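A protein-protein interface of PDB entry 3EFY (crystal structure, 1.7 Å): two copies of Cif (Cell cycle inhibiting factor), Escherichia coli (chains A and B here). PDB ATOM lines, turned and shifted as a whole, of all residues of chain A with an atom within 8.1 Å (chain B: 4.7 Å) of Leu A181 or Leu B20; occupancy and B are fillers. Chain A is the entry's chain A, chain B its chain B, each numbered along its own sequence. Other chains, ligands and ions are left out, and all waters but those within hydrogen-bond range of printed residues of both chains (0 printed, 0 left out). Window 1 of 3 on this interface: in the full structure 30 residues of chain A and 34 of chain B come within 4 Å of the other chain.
The backbone carbonyl oxygen of Ile B178 is in hydrogen-bond range of the side-chain sulfur of Cys A182 (3.4 Å).
Ile B178 touches its own counterpart, Ile A178.
Positions printed for both chains: 19, 174, 175 and 178.
Of the 14 pairs that touch across the chains among the printed residues, 1 has its exchanged pair printed and touching as well.
The side-chain sulfur of Cys A182 sits at hydrogen-bond distance from the backbone carbonyl oxygen of Ile A178 (3.4 Å).
O of Ser A180 lies within hydrogen-bond range of OG of Ser A183 (2.7 Å).
The backbone carbonyl oxygen (O) of Leu B20 is in hydrogen-bond range of the side-chain amide nitrogen (ND2) of Asn B174 (2.9 Å).
The backbone carbonyl oxygen (O) of Phe B21 sits close to the side-chain amide oxygen (OD1) of Asn B170.
Printed residues of chain A that touch a printed residue of chain B: Ile A177, Ile A178, Ser A180, Leu A181, Cys A182, Gly A184, Ala A185 and Leu A188.
Of the 13 printed residues of chain B, 7 touch a printed residue of chain A.
Hydrophobic or aromatic side chains of chain B within 4 Å of the printed part of chain A: Ala B16, Ile B17, Leu B20, Phe B21, Phe B99, Ile B175 and Ile B178.
Among the printed residues, 14 pairs touch across the chains.
Leu A181 touches five residues of chain B.
Of the printed residues of chain B, Gly A184 touches Phe B99.
Printed residues of chain B within 4 Å of Ala A185: Ile B175 (3.98 Å).
Of the printed residues of chain A, Ile B17 touches Leu A181.
Leu B20 touches just these residues of chain A: Leu A181 and Leu A188.
Of the printed residues of chain A, Phe B99 touches Ser A180 (3.3 Å), Leu A181 (3.9 Å) and Gly A184 (3.9 Å).
Asn B174 touches none of the printed residues of chain A.
Printed residues of chain A within 4 Å of Ile B178: Ile A178 (3.6 Å), Leu A181 (3.8 Å) and Cys A182 (3.4 Å).
The nearest printed residue of chain B that does not touch Leu A181 is Ile B175 (6.7 Å).
The nearest residue of chain A that does not touch Leu B20 is Ala A185 (6.4 Å).
The nearest printed residue of chain B that does not touch Cys A182 is Ile B175 (5.5 Å).
Among the printed residues, merely in contact across the chains: Ile A177 with Ala B16, Ile A178 with Ile B178, Ser A180 with Phe B99, Leu A181 with Ala B16, Leu A181 with Ile B17, Leu A181 with Leu B20, Leu A181 with Phe B99, Leu A181 with Ile B178, Gly A184 with Phe B99, Ala A185 with Ile B175, Leu A188 with Leu B20, Leu A188 with Phe B21 and Leu A188 with Ile B175.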
ATOM      1  N   LYS A  19       1.359 -13.017  11.513  1.00  0.00           N
ATOM      2  CA  LYS A  19       1.978 -11.782  10.991  1.00  0.00           C
ATOM      3  C   LYS A  19       1.009 -10.586  11.143  1.00  0.00           C
ATOM      4  O   LYS A  19       1.421  -9.470  11.523  1.00  0.00           O
ATOM      5  CB  LYS A  19       2.387 -11.934   9.532  1.00  0.00           C
ATOM      6  CG  LYS A  19       3.507 -12.951   9.330  1.00  0.00           C
ATOM      7  CD  LYS A  19       3.926 -13.004   7.856  1.00  0.00           C
ATOM      8  CE  LYS A  19       5.057 -14.045   7.603  1.00  0.00           C
ATOM      9  NZ  LYS A  19       5.249 -14.308   6.111  1.00  0.00           N
ATOM     10  N   ASN A 174      -2.538  -3.539  10.691  1.00  0.00           N
ATOM     11  CA  ASN A 174      -2.216  -4.536   9.677  1.00  0.00           C
ATOM     12  C   ASN A 174      -3.384  -4.988   8.797  1.00  0.00           C
ATOM     13  O   ASN A 174      -3.191  -5.326   7.636  1.00  0.00           O
ATOM     14  CB  ASN A 174      -1.497  -5.741  10.306  1.00  0.00           C
ATOM     15  CG  ASN A 174      -0.078  -5.379  10.782  1.00  0.00           C
ATOM     16  OD1 ASN A 174       0.541  -4.445  10.262  1.00  0.00           O
ATOM     17  ND2 ASN A 174       0.430  -6.113  11.758  1.00  0.00           N
ATOM     18  N   ILE A 175      -4.595  -4.971   9.345  1.00  0.00           N
ATOM     19  CA  ILE A 175      -5.776  -5.305   8.539  1.00  0.00           C
ATOM     20  C   ILE A 175      -6.022  -4.192   7.543  1.00  0.00           C
ATOM     21  O   ILE A 175      -6.322  -4.463   6.403  1.00  0.00           O
ATOM     22  CB  ILE A 175      -7.005  -5.542   9.383  1.00  0.00           C
ATOM     23  CG1 ILE A 175      -6.859  -6.850  10.172  1.00  0.00           C
ATOM     24  CG2 ILE A 175      -8.277  -5.622   8.478  1.00  0.00           C
ATOM     25  CD1 ILE A 175      -7.869  -7.012  11.292  1.00  0.00           C
ATOM     26  N   GLU A 176      -5.867  -2.939   7.969  1.00  0.00           N
ATOM     27  CA  GLU A 176      -5.964  -1.837   7.009  1.00  0.00           C
ATOM     28  C   GLU A 176      -4.951  -1.978   5.871  1.00  0.00           C
ATOM     29  O   GLU A 176      -5.249  -1.742   4.707  1.00  0.00           O
ATOM     30  CB  GLU A 176      -5.861  -0.480   7.712  1.00  0.00           C
ATOM     31  CG  GLU A 176      -7.065  -0.175   8.575  1.00  0.00           C
ATOM     32  CD  GLU A 176      -8.385  -0.269   7.792  1.00  0.00           C
ATOM     33  OE1 GLU A 176      -8.503   0.392   6.723  1.00  0.00           O
ATOM     34  OE2 GLU A 176      -9.298  -1.014   8.226  1.00  0.00           O
ATOM     35  N   ILE A 177      -3.723  -2.382   6.202  1.00  0.00           N
ATOM     36  CA  ILE A 177      -2.722  -2.595   5.189  1.00  0.00           C
ATOM     37  C   ILE A 177      -3.081  -3.711   4.222  1.00  0.00           C
ATOM     38  O   ILE A 177      -2.977  -3.528   2.997  1.00  0.00           O
ATOM     39  CB  ILE A 177      -1.316  -2.835   5.858  1.00  0.00           C
ATOM     40  CG1 ILE A 177      -0.833  -1.592   6.607  1.00  0.00           C
ATOM     41  CG2 ILE A 177      -0.328  -3.287   4.808  1.00  0.00           C
ATOM     42  CD1 ILE A 177       0.147  -1.941   7.746  1.00  0.00           C
ATOM     43  N   ILE A 178      -3.532  -4.859   4.722  1.00  0.00           N
ATOM     44  CA  ILE A 178      -3.863  -5.965   3.833  1.00  0.00           C
ATOM     45  C   ILE A 178      -5.028  -5.605   2.875  1.00  0.00           C
ATOM     46  O   ILE A 178      -4.980  -5.978   1.699  1.00  0.00           O
ATOM     47  CB  ILE A 178      -4.034  -7.294   4.611  1.00  0.00           C
ATOM     48  CG1 ILE A 178      -3.827  -8.508   3.702  1.00  0.00           C
ATOM     49  CG2 ILE A 178      -5.335  -7.374   5.295  1.00  0.00           C
ATOM     50  CD1 ILE A 178      -3.738  -9.846   4.489  1.00  0.00           C
ATOM     51  N   LYS A 179      -5.992  -4.835   3.359  1.00  0.00           N
ATOM     52  CA  LYS A 179      -7.141  -4.466   2.522  1.00  0.00           C
ATOM     53  C   LYS A 179      -6.655  -3.530   1.432  1.00  0.00           C
ATOM     54  O   LYS A 179      -7.037  -3.679   0.275  1.00  0.00           O
ATOM     55  CB  LYS A 179      -8.236  -3.783   3.340  1.00  0.00           C
ATOM     56  CG  LYS A 179      -8.911  -4.694   4.317  1.00  0.00           C
ATOM     57  CD  LYS A 179     -10.178  -4.067   4.901  1.00  0.00           C
ATOM     58  CE  LYS A 179      -9.872  -3.018   5.905  1.00  0.00           C
ATOM     59  NZ  LYS A 179     -11.145  -2.356   6.411  1.00  0.00           N
ATOM     60  N   SER A 180      -5.762  -2.618   1.815  1.00  0.00           N
ATOM     61  CA  SER A 180      -5.168  -1.673   0.836  1.00  0.00           C
ATOM     62  C   SER A 180      -4.365  -2.432  -0.242  1.00  0.00           C
ATOM     63  O   SER A 180      -4.513  -2.213  -1.461  1.00  0.00           O
ATOM     64  CB  SER A 180      -4.342  -0.613   1.556  1.00  0.00           C
ATOM     65  OG  SER A 180      -3.870   0.338   0.640  1.00  0.00           O
ATOM     66  N   LEU A 181      -3.506  -3.342   0.196  1.00  0.00           N
ATOM     67  CA  LEU A 181      -2.695  -4.092  -0.718  1.00  0.00           C
ATOM     68  C   LEU A 181      -3.542  -4.900  -1.688  1.00  0.00           C
ATOM     69  O   LEU A 181      -3.269  -4.912  -2.891  1.00  0.00           O
ATOM     70  CB  LEU A 181      -1.747  -5.026   0.047  1.00  0.00           C
ATOM     71  CG  LEU A 181      -0.590  -4.407   0.775  1.00  0.00           C
ATOM     72  CD1 LEU A 181       0.129  -5.545   1.551  1.00  0.00           C
ATOM     73  CD2 LEU A 181       0.330  -3.777  -0.208  1.00  0.00           C
ATOM     74  N   CYS A 182      -4.576  -5.570  -1.178  1.00  0.00           N
ATOM     75  CA  CYS A 182      -5.482  -6.313  -2.050  1.00  0.00           C
ATOM     76  C   CYS A 182      -6.122  -5.409  -3.117  1.00  0.00           C
ATOM     77  O   CYS A 182      -6.233  -5.814  -4.277  1.00  0.00           O
ATOM     78  CB  CYS A 182      -6.552  -7.040  -1.226  1.00  0.00           C
ATOM     79  SG  CYS A 182      -5.910  -8.502  -0.373  1.00  0.00           S
ATOM     80  N   SER A 183      -6.484  -4.196  -2.736  1.00  0.00           N
ATOM     81  CA  SER A 183      -7.127  -3.251  -3.662  1.00  0.00           C
ATOM     82  C   SER A 183      -6.224  -2.855  -4.836  1.00  0.00           C
ATOM     83  O   SER A 183      -6.727  -2.549  -5.922  1.00  0.00           O
ATOM     84  CB  SER A 183      -7.672  -2.036  -2.923  1.00  0.00           C
ATOM     85  OG  SER A 183      -6.677  -1.071  -2.629  1.00  0.00           O
ATOM     86  N   GLY A 184      -4.903  -2.886  -4.632  1.00  0.00           N
ATOM     87  CA  GLY A 184      -3.948  -2.555  -5.678  1.00  0.00           C
ATOM     88  C   GLY A 184      -3.168  -3.710  -6.287  1.00  0.00           C
ATOM     89  O   GLY A 184      -2.255  -3.512  -7.057  1.00  0.00           O
ATOM     90  N   ALA A 185      -3.530  -4.946  -5.946  1.00  0.00           N
ATOM     91  CA  ALA A 185      -2.690  -6.098  -6.233  1.00  0.00           C
ATOM     92  C   ALA A 185      -2.465  -6.387  -7.699  1.00  0.00           C
ATOM     93  O   ALA A 185      -1.394  -6.873  -8.059  1.00  0.00           O
ATOM     94  CB  ALA A 185      -3.230  -7.352  -5.514  1.00  0.00           C
ATOM     95  N   ALA A 186      -3.431  -6.051  -8.567  1.00  0.00           N
ATOM     96  CA  ALA A 186      -3.264  -6.322  -9.980  1.00  0.00           C
ATOM     97  C   ALA A 186      -2.005  -5.637 -10.550  1.00  0.00           C
ATOM     98  O   ALA A 186      -1.350  -6.154 -11.435  1.00  0.00           O
ATOM     99  CB  ALA A 186      -4.560  -5.892 -10.776  1.00  0.00           C
ATOM    100  N   ALA A 187      -1.665  -4.467 -10.031  1.00  0.00           N
ATOM    101  CA  ALA A 187      -0.532  -3.706 -10.551  1.00  0.00           C
ATOM    102  C   ALA A 187       0.841  -4.255 -10.076  1.00  0.00           C
ATOM    103  O   ALA A 187       1.907  -3.785 -10.559  1.00  0.00           O
ATOM    104  CB  ALA A 187      -0.667  -2.220 -10.156  1.00  0.00           C
ATOM    105  N   LEU A 188       0.832  -5.210  -9.146  1.00  0.00           N
ATOM    106  CA  LEU A 188       2.088  -5.720  -8.575  1.00  0.00           C
ATOM    107  C   LEU A 188       2.710  -6.844  -9.392  1.00  0.00           C
ATOM    108  O   LEU A 188       3.869  -7.194  -9.148  1.00  0.00           O
ATOM    109  CB  LEU A 188       1.858  -6.202  -7.138  1.00  0.00           C
ATOM    110  CG  LEU A 188       1.509  -5.179  -6.092  1.00  0.00           C
ATOM    111  CD1 LEU A 188       1.080  -5.822  -4.766  1.00  0.00           C
ATOM    112  CD2 LEU A 188       2.699  -4.215  -5.917  1.00  0.00           C
ATOM    113  N   ALA B  16       5.271  -3.379   3.592  1.00  0.00           N
ATOM    114  CA  ALA B  16       4.352  -4.446   3.303  1.00  0.00           C
ATOM    115  C   ALA B  16       4.496  -4.997   1.913  1.00  0.00           C
ATOM    116  O   ALA B  16       4.410  -6.204   1.744  1.00  0.00           O
ATOM    117  CB  ALA B  16       2.897  -3.957   3.553  1.00  0.00           C
ATOM    118  N   ILE B  17       4.768  -4.126   0.933  1.00  0.00           N
ATOM    119  CA  ILE B  17       5.008  -4.573  -0.452  1.00  0.00           C
ATOM    120  C   ILE B  17       6.308  -5.415  -0.485  1.00  0.00           C
ATOM    121  O   ILE B  17       6.365  -6.461  -1.151  1.00  0.00           O
ATOM    122  CB  ILE B  17       5.059  -3.389  -1.414  1.00  0.00           C
ATOM    123  CG1 ILE B  17       3.670  -2.746  -1.496  1.00  0.00           C
ATOM    124  CG2 ILE B  17       5.580  -3.813  -2.818  1.00  0.00           C
ATOM    125  CD1 ILE B  17       3.685  -1.416  -2.172  1.00  0.00           C
ATOM    126  N   MET B  18       7.328  -4.981   0.252  1.00  0.00           N
ATOM    127  CA  MET B  18       8.592  -5.769   0.281  1.00  0.00           C
ATOM    128  C   MET B  18       8.331  -7.178   0.770  1.00  0.00           C
ATOM    129  O   MET B  18       8.865  -8.156   0.268  1.00  0.00           O
ATOM    130  CB  MET B  18       9.645  -5.073   1.140  1.00  0.00           C
ATOM    131  CG  MET B  18      10.201  -3.789   0.527  1.00  0.00           C
ATOM    132  SD  MET B  18      10.983  -3.933  -1.112  1.00  0.00           S
ATOM    133  CE  MET B  18      12.641  -4.515  -0.621  1.00  0.00           C
ATOM    134  N   LYS B  19       7.476  -7.285   1.785  1.00  0.00           N
ATOM    135  CA  LYS B  19       7.110  -8.582   2.330  1.00  0.00           C
ATOM    136  C   LYS B  19       6.372  -9.447   1.308  1.00  0.00           C
ATOM    137  O   LYS B  19       6.624 -10.654   1.221  1.00  0.00           O
ATOM    138  CB  LYS B  19       6.312  -8.436   3.620  1.00  0.00           C
ATOM    139  CG  LYS B  19       7.096  -7.774   4.759  1.00  0.00           C
ATOM    140  CD  LYS B  19       6.296  -7.689   6.051  1.00  0.00           C
ATOM    141  CE  LYS B  19       6.299  -9.056   6.798  1.00  0.00           C
ATOM    142  NZ  LYS B  19       7.569  -9.955   6.987  1.00  0.00           N
ATOM    143  N   LEU B  20       5.477  -8.844   0.526  1.00  0.00           N
ATOM    144  CA  LEU B  20       4.830  -9.596  -0.540  1.00  0.00           C
ATOM    145  C   LEU B  20       5.804 -10.161  -1.544  1.00  0.00           C
ATOM    146  O   LEU B  20       5.674 -11.275  -1.997  1.00  0.00           O
ATOM    147  CB  LEU B  20       3.800  -8.742  -1.254  1.00  0.00           C
ATOM    148  CG  LEU B  20       2.541  -8.333  -0.502  1.00  0.00           C
ATOM    149  CD1 LEU B  20       1.641  -7.417  -1.385  1.00  0.00           C
ATOM    150  CD2 LEU B  20       1.782  -9.637  -0.090  1.00  0.00           C
ATOM    151  N   PHE B  21       6.808  -9.377  -1.923  1.00  0.00           N
ATOM    152  CA  PHE B  21       7.806  -9.900  -2.851  1.00  0.00           C
ATOM    153  C   PHE B  21       8.738 -10.944  -2.260  1.00  0.00           C
ATOM    154  O   PHE B  21       9.185 -11.843  -2.971  1.00  0.00           O
ATOM    155  CB  PHE B  21       8.639  -8.748  -3.414  1.00  0.00           C
ATOM    156  CG  PHE B  21       7.956  -8.005  -4.522  1.00  0.00           C
ATOM    157  CD1 PHE B  21       8.111  -8.396  -5.839  1.00  0.00           C
ATOM    158  CD2 PHE B  21       7.135  -6.907  -4.243  1.00  0.00           C
ATOM    159  CE1 PHE B  21       7.474  -7.702  -6.869  1.00  0.00           C
ATOM    160  CE2 PHE B  21       6.510  -6.208  -5.253  1.00  0.00           C
ATOM    161  CZ  PHE B  21       6.643  -6.647  -6.578  1.00  0.00           C
ATOM    162  N   LEU B  22       9.078 -10.809  -0.993  1.00  0.00           N
ATOM    163  CA  LEU B  22      10.220 -11.518  -0.448  1.00  0.00           C
ATOM    164  C   LEU B  22       9.964 -12.608   0.601  1.00  0.00           C
ATOM    165  O   LEU B  22      10.822 -13.497   0.784  1.00  0.00           O
ATOM    166  CB  LEU B  22      11.218 -10.492   0.103  1.00  0.00           C
ATOM    167  CG  LEU B  22      11.698  -9.443  -0.888  1.00  0.00           C
ATOM    168  CD1 LEU B  22      12.532  -8.396  -0.157  1.00  0.00           C
ATOM    169  CD2 LEU B  22      12.493 -10.070  -2.079  1.00  0.00           C
ATOM    170  N   PHE B  99      -3.154   4.338  -2.042  1.00  0.00           N
ATOM    171  CA  PHE B  99      -2.593   3.234  -2.790  1.00  0.00           C
ATOM    172  C   PHE B  99      -3.541   2.690  -3.860  1.00  0.00           C
ATOM    173  O   PHE B  99      -3.148   2.492  -4.985  1.00  0.00           O
ATOM    174  CB  PHE B  99      -2.191   2.115  -1.820  1.00  0.00           C
ATOM    175  CG  PHE B  99      -1.450   0.966  -2.453  1.00  0.00           C
ATOM    176  CD1 PHE B  99      -0.113   1.087  -2.836  1.00  0.00           C
ATOM    177  CD2 PHE B  99      -2.051  -0.264  -2.578  1.00  0.00           C
ATOM    178  CE1 PHE B  99       0.562   0.015  -3.350  1.00  0.00           C
ATOM    179  CE2 PHE B  99      -1.344  -1.361  -3.103  1.00  0.00           C
ATOM    180  CZ  PHE B  99      -0.020  -1.206  -3.461  1.00  0.00           C
ATOM    181  N   ASN B 170       7.039 -16.130  -6.134  1.00  0.00           N
ATOM    182  CA  ASN B 170       6.887 -15.815  -4.746  1.00  0.00           C
ATOM    183  C   ASN B 170       5.908 -14.672  -4.519  1.00  0.00           C
ATOM    184  O   ASN B 170       5.062 -14.756  -3.630  1.00  0.00           O
ATOM    185  CB  ASN B 170       8.228 -15.490  -4.113  1.00  0.00           C
ATOM    186  CG  ASN B 170       8.169 -15.574  -2.642  1.00  0.00           C
ATOM    187  OD1 ASN B 170       8.351 -14.573  -1.910  1.00  0.00           O
ATOM    188  ND2 ASN B 170       7.905 -16.797  -2.153  1.00  0.00           N
ATOM    189  N   ILE B 171       5.991 -13.608  -5.324  1.00  0.00           N
ATOM    190  CA  ILE B 171       5.020 -12.522  -5.232  1.00  0.00           C
ATOM    191  C   ILE B 171       3.621 -13.035  -5.606  1.00  0.00           C
ATOM    192  O   ILE B 171       2.663 -12.720  -4.930  1.00  0.00           O
ATOM    193  CB  ILE B 171       5.440 -11.239  -6.048  1.00  0.00           C
ATOM    194  CG1 ILE B 171       4.342 -10.165  -6.028  1.00  0.00           C
ATOM    195  CG2 ILE B 171       5.778 -11.560  -7.484  1.00  0.00           C
ATOM    196  CD1 ILE B 171       4.117  -9.556  -4.742  1.00  0.00           C
ATOM    197  N   ASN B 174       2.304 -14.977  -2.509  1.00  0.00           N
ATOM    198  CA  ASN B 174       1.964 -14.113  -1.403  1.00  0.00           C
ATOM    199  C   ASN B 174       0.714 -13.262  -1.644  1.00  0.00           C
ATOM    200  O   ASN B 174      -0.027 -12.985  -0.733  1.00  0.00           O
ATOM    201  CB  ASN B 174       3.182 -13.231  -1.014  1.00  0.00           C
ATOM    202  CG  ASN B 174       4.222 -14.037  -0.290  1.00  0.00           C
ATOM    203  OD1 ASN B 174       3.905 -15.073   0.305  1.00  0.00           O
ATOM    204  ND2 ASN B 174       5.460 -13.603  -0.331  1.00  0.00           N
ATOM    205  N   ILE B 175       0.498 -12.858  -2.890  1.00  0.00           N
ATOM    206  CA  ILE B 175      -0.710 -12.158  -3.241  1.00  0.00           C
ATOM    207  C   ILE B 175      -1.928 -13.089  -3.070  1.00  0.00           C
ATOM    208  O   ILE B 175      -2.963 -12.653  -2.573  1.00  0.00           O
ATOM    209  CB  ILE B 175      -0.630 -11.558  -4.625  1.00  0.00           C
ATOM    210  CG1 ILE B 175       0.307 -10.326  -4.587  1.00  0.00           C
ATOM    211  CG2 ILE B 175      -2.047 -11.137  -5.129  1.00  0.00           C
ATOM    212  CD1 ILE B 175       0.698  -9.795  -5.938  1.00  0.00           C
ATOM    213  N   ILE B 178      -2.743 -13.142   0.711  1.00  0.00           N
ATOM    214  CA  ILE B 178      -3.394 -12.002   1.247  1.00  0.00           C
ATOM    215  C   ILE B 178      -4.850 -11.874   0.733  1.00  0.00           C
ATOM    216  O   ILE B 178      -5.708 -11.404   1.480  1.00  0.00           O
ATOM    217  CB  ILE B 178      -2.638 -10.662   1.112  1.00  0.00           C
ATOM    218  CG1 ILE B 178      -2.409 -10.246  -0.333  1.00  0.00           C
ATOM    219  CG2 ILE B 178      -1.314 -10.733   1.918  1.00  0.00           C
ATOM    220  CD1 ILE B 178      -1.941  -8.768  -0.437  1.00  0.00           C
